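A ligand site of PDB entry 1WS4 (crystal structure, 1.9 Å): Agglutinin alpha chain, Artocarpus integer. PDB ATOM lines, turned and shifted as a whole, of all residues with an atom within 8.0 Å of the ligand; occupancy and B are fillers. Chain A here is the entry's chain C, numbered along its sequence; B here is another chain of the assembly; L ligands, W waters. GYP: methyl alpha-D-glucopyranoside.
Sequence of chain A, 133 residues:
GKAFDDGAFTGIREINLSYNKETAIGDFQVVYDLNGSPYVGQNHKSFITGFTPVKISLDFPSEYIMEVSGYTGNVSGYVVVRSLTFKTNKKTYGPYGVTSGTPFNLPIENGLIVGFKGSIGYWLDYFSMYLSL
The side-chain carboxylate (OD2) of Asp 125 lies within hydrogen-bond range of the backbone NH (N) of Gly 1 (3.2 Å).
O of Gly 1 sits close to OG of Ser 119 (3.4 Å).
The backbone NH (N) of Asp 125 sits at hydrogen-bond distance from the backbone carbonyl oxygen (O) of Ser 119.
N of Ala 17 of chain B is in hydrogen-bond range of O of Asp 125, 2.8 Å away.
O of Tyr 122 sits at hydrogen-bond distance from OG of Ser 46 (2.5 Å).
The backbone NH (N) of Phe 47 sits at hydrogen-bond distance from the backbone carbonyl oxygen (O) of Gly 121.
Tyr 78 touches the ligand.
CA of Gly 121 touches O6 of the ligand, at 3.5 Å.
Hydrophobic or aromatic side chains that line the ligand: Tyr 78, Tyr 122 and Trp 123.
Water W2 bridges N of Gly 1 (3.3 Å) and O3 of the ligand (3.4 Å).
Water W1 lies within hydrogen-bond range of O of Val 79 (2.8 Å), OD1 of Asp 125 (2.9 Å) and O4 of the ligand (3.4 Å).
The backbone NH (N) of Gly 1 is in hydrogen-bond range of an oxygen (O3) of the ligand, 2.8 Å away.
The side-chain carboxylate of Asp 125 lies within hydrogen-bond range of an oxygen (O6) of the ligand.
O6 of the ligand lies within hydrogen-bond range of N of Trp 123 (2.9 Å).
O of Trp 123 is in hydrogen-bond range of O6 of the ligand (3.0 Å).
An oxygen (O6) of the ligand is in hydrogen-bond range of the backbone NH (N) of Tyr 122.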
ATOM      1  N   GLY A   1     -11.120 -14.106  -6.878  1.00  0.00           N
ATOM      2  CA  GLY A   1     -12.521 -13.904  -7.329  1.00  0.00           C
ATOM      3  C   GLY A   1     -13.223 -12.807  -6.566  1.00  0.00           C
ATOM      4  O   GLY A   1     -12.584 -12.057  -5.832  1.00  0.00           O
ATOM      5  N   LYS A   2     -14.532 -12.719  -6.734  1.00  0.00           N
ATOM      6  CA  LYS A   2     -15.342 -11.705  -6.051  1.00  0.00           C
ATOM      7  C   LYS A   2     -15.728 -12.196  -4.663  1.00  0.00           C
ATOM      8  O   LYS A   2     -16.458 -13.183  -4.511  1.00  0.00           O
ATOM      9  CB  LYS A   2     -16.602 -11.428  -6.881  1.00  0.00           C
ATOM     10  CG  LYS A   2     -17.399 -10.220  -6.432  1.00  0.00           C
ATOM     11  CD  LYS A   2     -18.639 -10.047  -7.309  1.00  0.00           C
ATOM     12  CE  LYS A   2     -19.223  -8.644  -7.192  1.00  0.00           C
ATOM     13  NZ  LYS A   2     -19.544  -8.284  -5.789  1.00  0.00           N
ATOM     14  N   ALA A  24     -14.990 -27.892 -10.348  1.00  0.00           N
ATOM     15  CA  ALA A  24     -15.271 -27.603  -8.948  1.00  0.00           C
ATOM     16  C   ALA A  24     -16.651 -26.985  -8.745  1.00  0.00           C
ATOM     17  O   ALA A  24     -17.489 -26.996  -9.637  1.00  0.00           O
ATOM     18  CB  ALA A  24     -14.195 -26.671  -8.410  1.00  0.00           C
ATOM     19  N   ILE A  25     -16.864 -26.447  -7.551  1.00  0.00           N
ATOM     20  CA  ILE A  25     -18.133 -25.818  -7.206  1.00  0.00           C
ATOM     21  C   ILE A  25     -18.173 -24.431  -7.833  1.00  0.00           C
ATOM     22  O   ILE A  25     -17.168 -23.724  -7.853  1.00  0.00           O
ATOM     23  CB  ILE A  25     -18.269 -25.732  -5.675  1.00  0.00           C
ATOM     24  CG1 ILE A  25     -18.426 -27.159  -5.127  1.00  0.00           C
ATOM     25  CG2 ILE A  25     -19.472 -24.875  -5.300  1.00  0.00           C
ATOM     26  CD1 ILE A  25     -17.917 -27.321  -3.734  1.00  0.00           C
ATOM     27  N   SER A  46     -20.726 -17.777 -10.369  1.00  0.00           N
ATOM     28  CA  SER A  46     -19.439 -17.991 -11.003  1.00  0.00           C
ATOM     29  C   SER A  46     -19.345 -17.049 -12.202  1.00  0.00           C
ATOM     30  O   SER A  46     -20.376 -16.638 -12.747  1.00  0.00           O
ATOM     31  CB  SER A  46     -19.334 -19.440 -11.479  1.00  0.00           C
ATOM     32  OG  SER A  46     -18.268 -19.580 -12.399  1.00  0.00           O
ATOM     33  N   PHE A  47     -18.117 -16.735 -12.627  1.00  0.00           N
ATOM     34  CA  PHE A  47     -17.904 -15.868 -13.784  1.00  0.00           C
ATOM     35  C   PHE A  47     -18.231 -16.589 -15.087  1.00  0.00           C
ATOM     36  O   PHE A  47     -18.375 -15.947 -16.128  1.00  0.00           O
ATOM     37  CB  PHE A  47     -16.443 -15.411 -13.865  1.00  0.00           C
ATOM     38  CG  PHE A  47     -15.998 -14.534 -12.728  1.00  0.00           C
ATOM     39  CD1 PHE A  47     -16.917 -13.877 -11.919  1.00  0.00           C
ATOM     40  CD2 PHE A  47     -14.633 -14.332 -12.488  1.00  0.00           C
ATOM     41  CE1 PHE A  47     -16.491 -13.013 -10.900  1.00  0.00           C
ATOM     42  CE2 PHE A  47     -14.199 -13.474 -11.478  1.00  0.00           C
ATOM     43  CZ  PHE A  47     -15.128 -12.814 -10.680  1.00  0.00           C
ATOM     44  N   ILE A  48     -18.334 -17.912 -15.027  1.00  0.00           N
ATOM     45  CA  ILE A  48     -18.640 -18.694 -16.221  1.00  0.00           C
ATOM     46  C   ILE A  48     -19.877 -19.572 -16.032  1.00  0.00           C
ATOM     47  O   ILE A  48     -20.484 -19.580 -14.955  1.00  0.00           O
ATOM     48  CB  ILE A  48     -17.456 -19.603 -16.617  1.00  0.00           C
ATOM     49  CG1 ILE A  48     -17.100 -20.551 -15.465  1.00  0.00           C
ATOM     50  CG2 ILE A  48     -16.241 -18.744 -16.962  1.00  0.00           C
ATOM     51  CD1 ILE A  48     -16.048 -21.584 -15.820  1.00  0.00           C
ATOM     52  N   VAL A  75      -7.175 -26.343  -9.750  1.00  0.00           N
ATOM     53  CA  VAL A  75      -7.956 -26.400 -10.985  1.00  0.00           C
ATOM     54  C   VAL A  75      -7.405 -25.275 -11.855  1.00  0.00           C
ATOM     55  O   VAL A  75      -7.579 -24.099 -11.534  1.00  0.00           O
ATOM     56  CB  VAL A  75      -9.462 -26.169 -10.732  1.00  0.00           C
ATOM     57  CG1 VAL A  75     -10.201 -26.079 -12.055  1.00  0.00           C
ATOM     58  CG2 VAL A  75     -10.029 -27.302  -9.891  1.00  0.00           C
ATOM     59  N   SER A  76      -6.738 -25.635 -12.942  1.00  0.00           N
ATOM     60  CA  SER A  76      -6.165 -24.648 -13.842  1.00  0.00           C
ATOM     61  C   SER A  76      -5.230 -23.677 -13.126  1.00  0.00           C
ATOM     62  O   SER A  76      -5.205 -22.489 -13.433  1.00  0.00           O
ATOM     63  CB  SER A  76      -7.271 -23.858 -14.551  1.00  0.00           C
ATOM     64  OG  SER A  76      -8.051 -24.707 -15.370  1.00  0.00           O
ATOM     65  N   GLY A  77      -4.482 -24.187 -12.156  1.00  0.00           N
ATOM     66  CA  GLY A  77      -3.556 -23.348 -11.419  1.00  0.00           C
ATOM     67  C   GLY A  77      -4.113 -22.646 -10.191  1.00  0.00           C
ATOM     68  O   GLY A  77      -3.378 -21.969  -9.473  1.00  0.00           O
ATOM     69  N   TYR A  78      -5.409 -22.802  -9.946  1.00  0.00           N
ATOM     70  CA  TYR A  78      -6.057 -22.157  -8.803  1.00  0.00           C
ATOM     71  C   TYR A  78      -6.505 -23.166  -7.758  1.00  0.00           C
ATOM     72  O   TYR A  78      -7.102 -24.189  -8.088  1.00  0.00           O
ATOM     73  CB  TYR A  78      -7.277 -21.358  -9.281  1.00  0.00           C
ATOM     74  CG  TYR A  78      -6.935 -20.212 -10.197  1.00  0.00           C
ATOM     75  CD1 TYR A  78      -6.450 -19.003  -9.693  1.00  0.00           C
ATOM     76  CD2 TYR A  78      -7.080 -20.336 -11.577  1.00  0.00           C
ATOM     77  CE1 TYR A  78      -6.115 -17.946 -10.544  1.00  0.00           C
ATOM     78  CE2 TYR A  78      -6.750 -19.289 -12.436  1.00  0.00           C
ATOM     79  CZ  TYR A  78      -6.266 -18.101 -11.918  1.00  0.00           C
ATOM     80  OH  TYR A  78      -5.947 -17.070 -12.774  1.00  0.00           O
ATOM     81  N   VAL A  79      -6.208 -22.885  -6.496  1.00  0.00           N
ATOM     82  CA  VAL A  79      -6.624 -23.762  -5.402  1.00  0.00           C
ATOM     83  C   VAL A  79      -8.061 -23.356  -5.080  1.00  0.00           C
ATOM     84  O   VAL A  79      -8.315 -22.214  -4.696  1.00  0.00           O
ATOM     85  CB  VAL A  79      -5.745 -23.560  -4.156  1.00  0.00           C
ATOM     86  CG1 VAL A  79      -6.228 -24.471  -3.021  1.00  0.00           C
ATOM     87  CG2 VAL A  79      -4.287 -23.873  -4.484  1.00  0.00           C
ATOM     88  N   VAL A  80      -8.999 -24.285  -5.254  1.00  0.00           N
ATOM     89  CA  VAL A  80     -10.406 -24.005  -4.996  1.00  0.00           C
ATOM     90  C   VAL A  80     -11.113 -25.139  -4.275  1.00  0.00           C
ATOM     91  O   VAL A  80     -10.534 -26.195  -4.039  1.00  0.00           O
ATOM     92  CB  VAL A  80     -11.165 -23.753  -6.332  1.00  0.00           C
ATOM     93  CG1 VAL A  80     -10.597 -22.519  -7.027  1.00  0.00           C
ATOM     94  CG2 VAL A  80     -11.041 -24.981  -7.229  1.00  0.00           C
ATOM     95  N   VAL A  81     -12.373 -24.904  -3.921  1.00  0.00           N
ATOM     96  CA  VAL A  81     -13.198 -25.906  -3.251  1.00  0.00           C
ATOM     97  C   VAL A  81     -13.804 -26.742  -4.371  1.00  0.00           C
ATOM     98  O   VAL A  81     -14.656 -26.267  -5.124  1.00  0.00           O
ATOM     99  CB  VAL A  81     -14.322 -25.242  -2.426  1.00  0.00           C
ATOM    100  CG1 VAL A  81     -15.174 -26.308  -1.744  1.00  0.00           C
ATOM    101  CG2 VAL A  81     -13.722 -24.301  -1.393  1.00  0.00           C
ATOM    102  N   SER A 119     -15.373 -16.455  -1.418  1.00  0.00           N
ATOM    103  CA  SER A 119     -15.044 -15.783  -2.666  1.00  0.00           C
ATOM    104  C   SER A 119     -15.289 -16.717  -3.841  1.00  0.00           C
ATOM    105  O   SER A 119     -15.010 -17.907  -3.753  1.00  0.00           O
ATOM    106  CB  SER A 119     -13.571 -15.345  -2.633  1.00  0.00           C
ATOM    107  OG  SER A 119     -13.174 -14.795  -3.878  1.00  0.00           O
ATOM    108  N   ILE A 120     -15.804 -16.171  -4.938  1.00  0.00           N
ATOM    109  CA  ILE A 120     -16.078 -16.959  -6.124  1.00  0.00           C
ATOM    110  C   ILE A 120     -15.622 -16.250  -7.398  1.00  0.00           C
ATOM    111  O   ILE A 120     -15.996 -15.104  -7.635  1.00  0.00           O
ATOM    112  CB  ILE A 120     -17.585 -17.280  -6.263  1.00  0.00           C
ATOM    113  CG1 ILE A 120     -18.068 -18.092  -5.051  1.00  0.00           C
ATOM    114  CG2 ILE A 120     -17.848 -18.049  -7.554  1.00  0.00           C
ATOM    115  CD1 ILE A 120     -19.554 -18.415  -5.080  1.00  0.00           C
ATOM    116  N   GLY A 121     -14.797 -16.928  -8.185  1.00  0.00           N
ATOM    117  CA  GLY A 121     -14.336 -16.387  -9.455  1.00  0.00           C
ATOM    118  C   GLY A 121     -14.934 -17.343 -10.445  1.00  0.00           C
ATOM    119  O   GLY A 121     -16.146 -17.385 -10.611  1.00  0.00           O
ATOM    120  N   TYR A 122     -14.102 -18.144 -11.112  1.00  0.00           N
ATOM    121  CA  TYR A 122     -14.656 -19.143 -12.008  1.00  0.00           C
ATOM    122  C   TYR A 122     -15.269 -20.196 -11.084  1.00  0.00           C
ATOM    123  O   TYR A 122     -16.289 -20.796 -11.393  1.00  0.00           O
ATOM    124  CB  TYR A 122     -13.574 -19.801 -12.871  1.00  0.00           C
ATOM    125  CG  TYR A 122     -13.201 -19.036 -14.117  1.00  0.00           C
ATOM    126  CD1 TYR A 122     -12.536 -19.673 -15.171  1.00  0.00           C
ATOM    127  CD2 TYR A 122     -13.511 -17.684 -14.258  1.00  0.00           C
ATOM    128  CE1 TYR A 122     -12.180 -18.974 -16.323  1.00  0.00           C
ATOM    129  CE2 TYR A 122     -13.163 -16.980 -15.411  1.00  0.00           C
ATOM    130  CZ  TYR A 122     -12.498 -17.636 -16.442  1.00  0.00           C
ATOM    131  OH  TYR A 122     -12.160 -16.950 -17.591  1.00  0.00           O
ATOM    132  N   TRP A 123     -14.619 -20.399  -9.940  1.00  0.00           N
ATOM    133  CA  TRP A 123     -15.065 -21.386  -8.958  1.00  0.00           C
ATOM    134  C   TRP A 123     -14.994 -20.819  -7.539  1.00  0.00           C
ATOM    135  O   TRP A 123     -14.498 -19.712  -7.325  1.00  0.00           O
ATOM    136  CB  TRP A 123     -14.193 -22.638  -9.052  1.00  0.00           C
ATOM    137  CG  TRP A 123     -14.138 -23.189 -10.433  1.00  0.00           C
ATOM    138  CD1 TRP A 123     -15.137 -23.818 -11.106  1.00  0.00           C
ATOM    139  CD2 TRP A 123     -13.048 -23.074 -11.365  1.00  0.00           C
ATOM    140  NE1 TRP A 123     -14.748 -24.101 -12.394  1.00  0.00           N
ATOM    141  CE2 TRP A 123     -13.470 -23.661 -12.579  1.00  0.00           C
ATOM    142  CE3 TRP A 123     -11.753 -22.542 -11.281  1.00  0.00           C
ATOM    143  CZ2 TRP A 123     -12.642 -23.713 -13.707  1.00  0.00           C
ATOM    144  CZ3 TRP A 123     -10.939 -22.597 -12.407  1.00  0.00           C
ATOM    145  CH2 TRP A 123     -11.387 -23.190 -13.609  1.00  0.00           C
ATOM    146  N   LEU A 124     -15.496 -21.588  -6.576  1.00  0.00           N
ATOM    147  CA  LEU A 124     -15.475 -21.163  -5.182  1.00  0.00           C
ATOM    148  C   LEU A 124     -14.028 -21.231  -4.693  1.00  0.00           C
ATOM    149  O   LEU A 124     -13.483 -22.324  -4.510  1.00  0.00           O
ATOM    150  CB  LEU A 124     -16.366 -22.079  -4.346  1.00  0.00           C
ATOM    151  CG  LEU A 124     -16.458 -21.822  -2.835  1.00  0.00           C
ATOM    152  CD1 LEU A 124     -17.018 -20.435  -2.555  1.00  0.00           C
ATOM    153  CD2 LEU A 124     -17.360 -22.895  -2.218  1.00  0.00           C
ATOM    154  N   ASP A 125     -13.408 -20.071  -4.498  1.00  0.00           N
ATOM    155  CA  ASP A 125     -12.020 -19.984  -4.059  1.00  0.00           C
ATOM    156  C   ASP A 125     -11.812 -20.456  -2.633  1.00  0.00           C
ATOM    157  O   ASP A 125     -10.865 -21.187  -2.336  1.00  0.00           O
ATOM    158  CB  ASP A 125     -11.529 -18.540  -4.181  1.00  0.00           C
ATOM    159  CG  ASP A 125     -11.636 -17.996  -5.596  1.00  0.00           C
ATOM    160  OD1 ASP A 125     -11.106 -18.643  -6.515  1.00  0.00           O
ATOM    161  OD2 ASP A 125     -12.245 -16.912  -5.782  1.00  0.00           O
ATOM    162  N   TYR A 126     -12.695 -20.030  -1.741  1.00  0.00           N
ATOM    163  CA  TYR A 126     -12.616 -20.406  -0.340  1.00  0.00           C
ATOM    164  C   TYR A 126     -13.880 -19.977   0.370  1.00  0.00           C
ATOM    165  O   TYR A 126     -14.665 -19.192  -0.172  1.00  0.00           O
ATOM    166  CB  TYR A 126     -11.408 -19.738   0.329  1.00  0.00           C
ATOM    167  CG  TYR A 126     -11.423 -18.224   0.280  1.00  0.00           C
ATOM    168  CD1 TYR A 126     -12.213 -17.486   1.177  1.00  0.00           C
ATOM    169  CD2 TYR A 126     -10.666 -17.533  -0.662  1.00  0.00           C
ATOM    170  CE1 TYR A 126     -12.247 -16.081   1.115  1.00  0.00           C
ATOM    171  CE2 TYR A 126     -10.697 -16.144  -0.731  1.00  0.00           C
ATOM    172  CZ  TYR A 126     -11.489 -15.429   0.159  1.00  0.00           C
ATOM    173  OH  TYR A 126     -11.519 -14.056   0.072  1.00  0.00           O
ATOM    174  N   ALA B  17      -8.383 -21.695  -1.136  1.00  0.00           N
ATOM    175  CA  ALA B  17      -7.215 -20.855  -1.424  1.00  0.00           C
ATOM    176  C   ALA B  17      -6.840 -20.016  -0.214  1.00  0.00           C
ATOM    177  O   ALA B  17      -7.707 -19.642   0.583  1.00  0.00           O
ATOM    178  CB  ALA B  17      -7.512 -19.964  -2.623  1.00  0.00           C
HETATM  179  C1  GYP L   1     -10.736 -16.499 -12.085  1.00  0.00           C
HETATM  180  C2  GYP L   1     -10.594 -15.311 -11.122  1.00  0.00           C
HETATM  181  C3  GYP L   1      -9.610 -15.619  -9.979  1.00  0.00           C
HETATM  182  C4  GYP L   1     -10.137 -16.843  -9.229  1.00  0.00           C
HETATM  183  C5  GYP L   1     -10.240 -18.043 -10.193  1.00  0.00           C
HETATM  184  C6  GYP L   1     -10.766 -19.304  -9.508  1.00  0.00           C
HETATM  185  C7  GYP L   1      -9.601 -17.820 -13.773  1.00  0.00           C
HETATM  186  O1  GYP L   1      -9.512 -16.723 -12.833  1.00  0.00           O
HETATM  187  O2  GYP L   1     -10.167 -14.158 -11.874  1.00  0.00           O
HETATM  188  O3  GYP L   1      -9.509 -14.482  -9.097  1.00  0.00           O
HETATM  189  O4  GYP L   1      -9.254 -17.163  -8.147  1.00  0.00           O
HETATM  190  O5  GYP L   1     -11.121 -17.699 -11.319  1.00  0.00           O
HETATM  191  O6  GYP L   1     -12.128 -19.142  -9.114  1.00  0.00           O
HETATM  192  O   HOH W   1      -8.521 -19.730  -5.996  1.00  0.00           O
HETATM  193  O   HOH W   2      -9.432 -11.388  -7.682  1.00  0.00           O
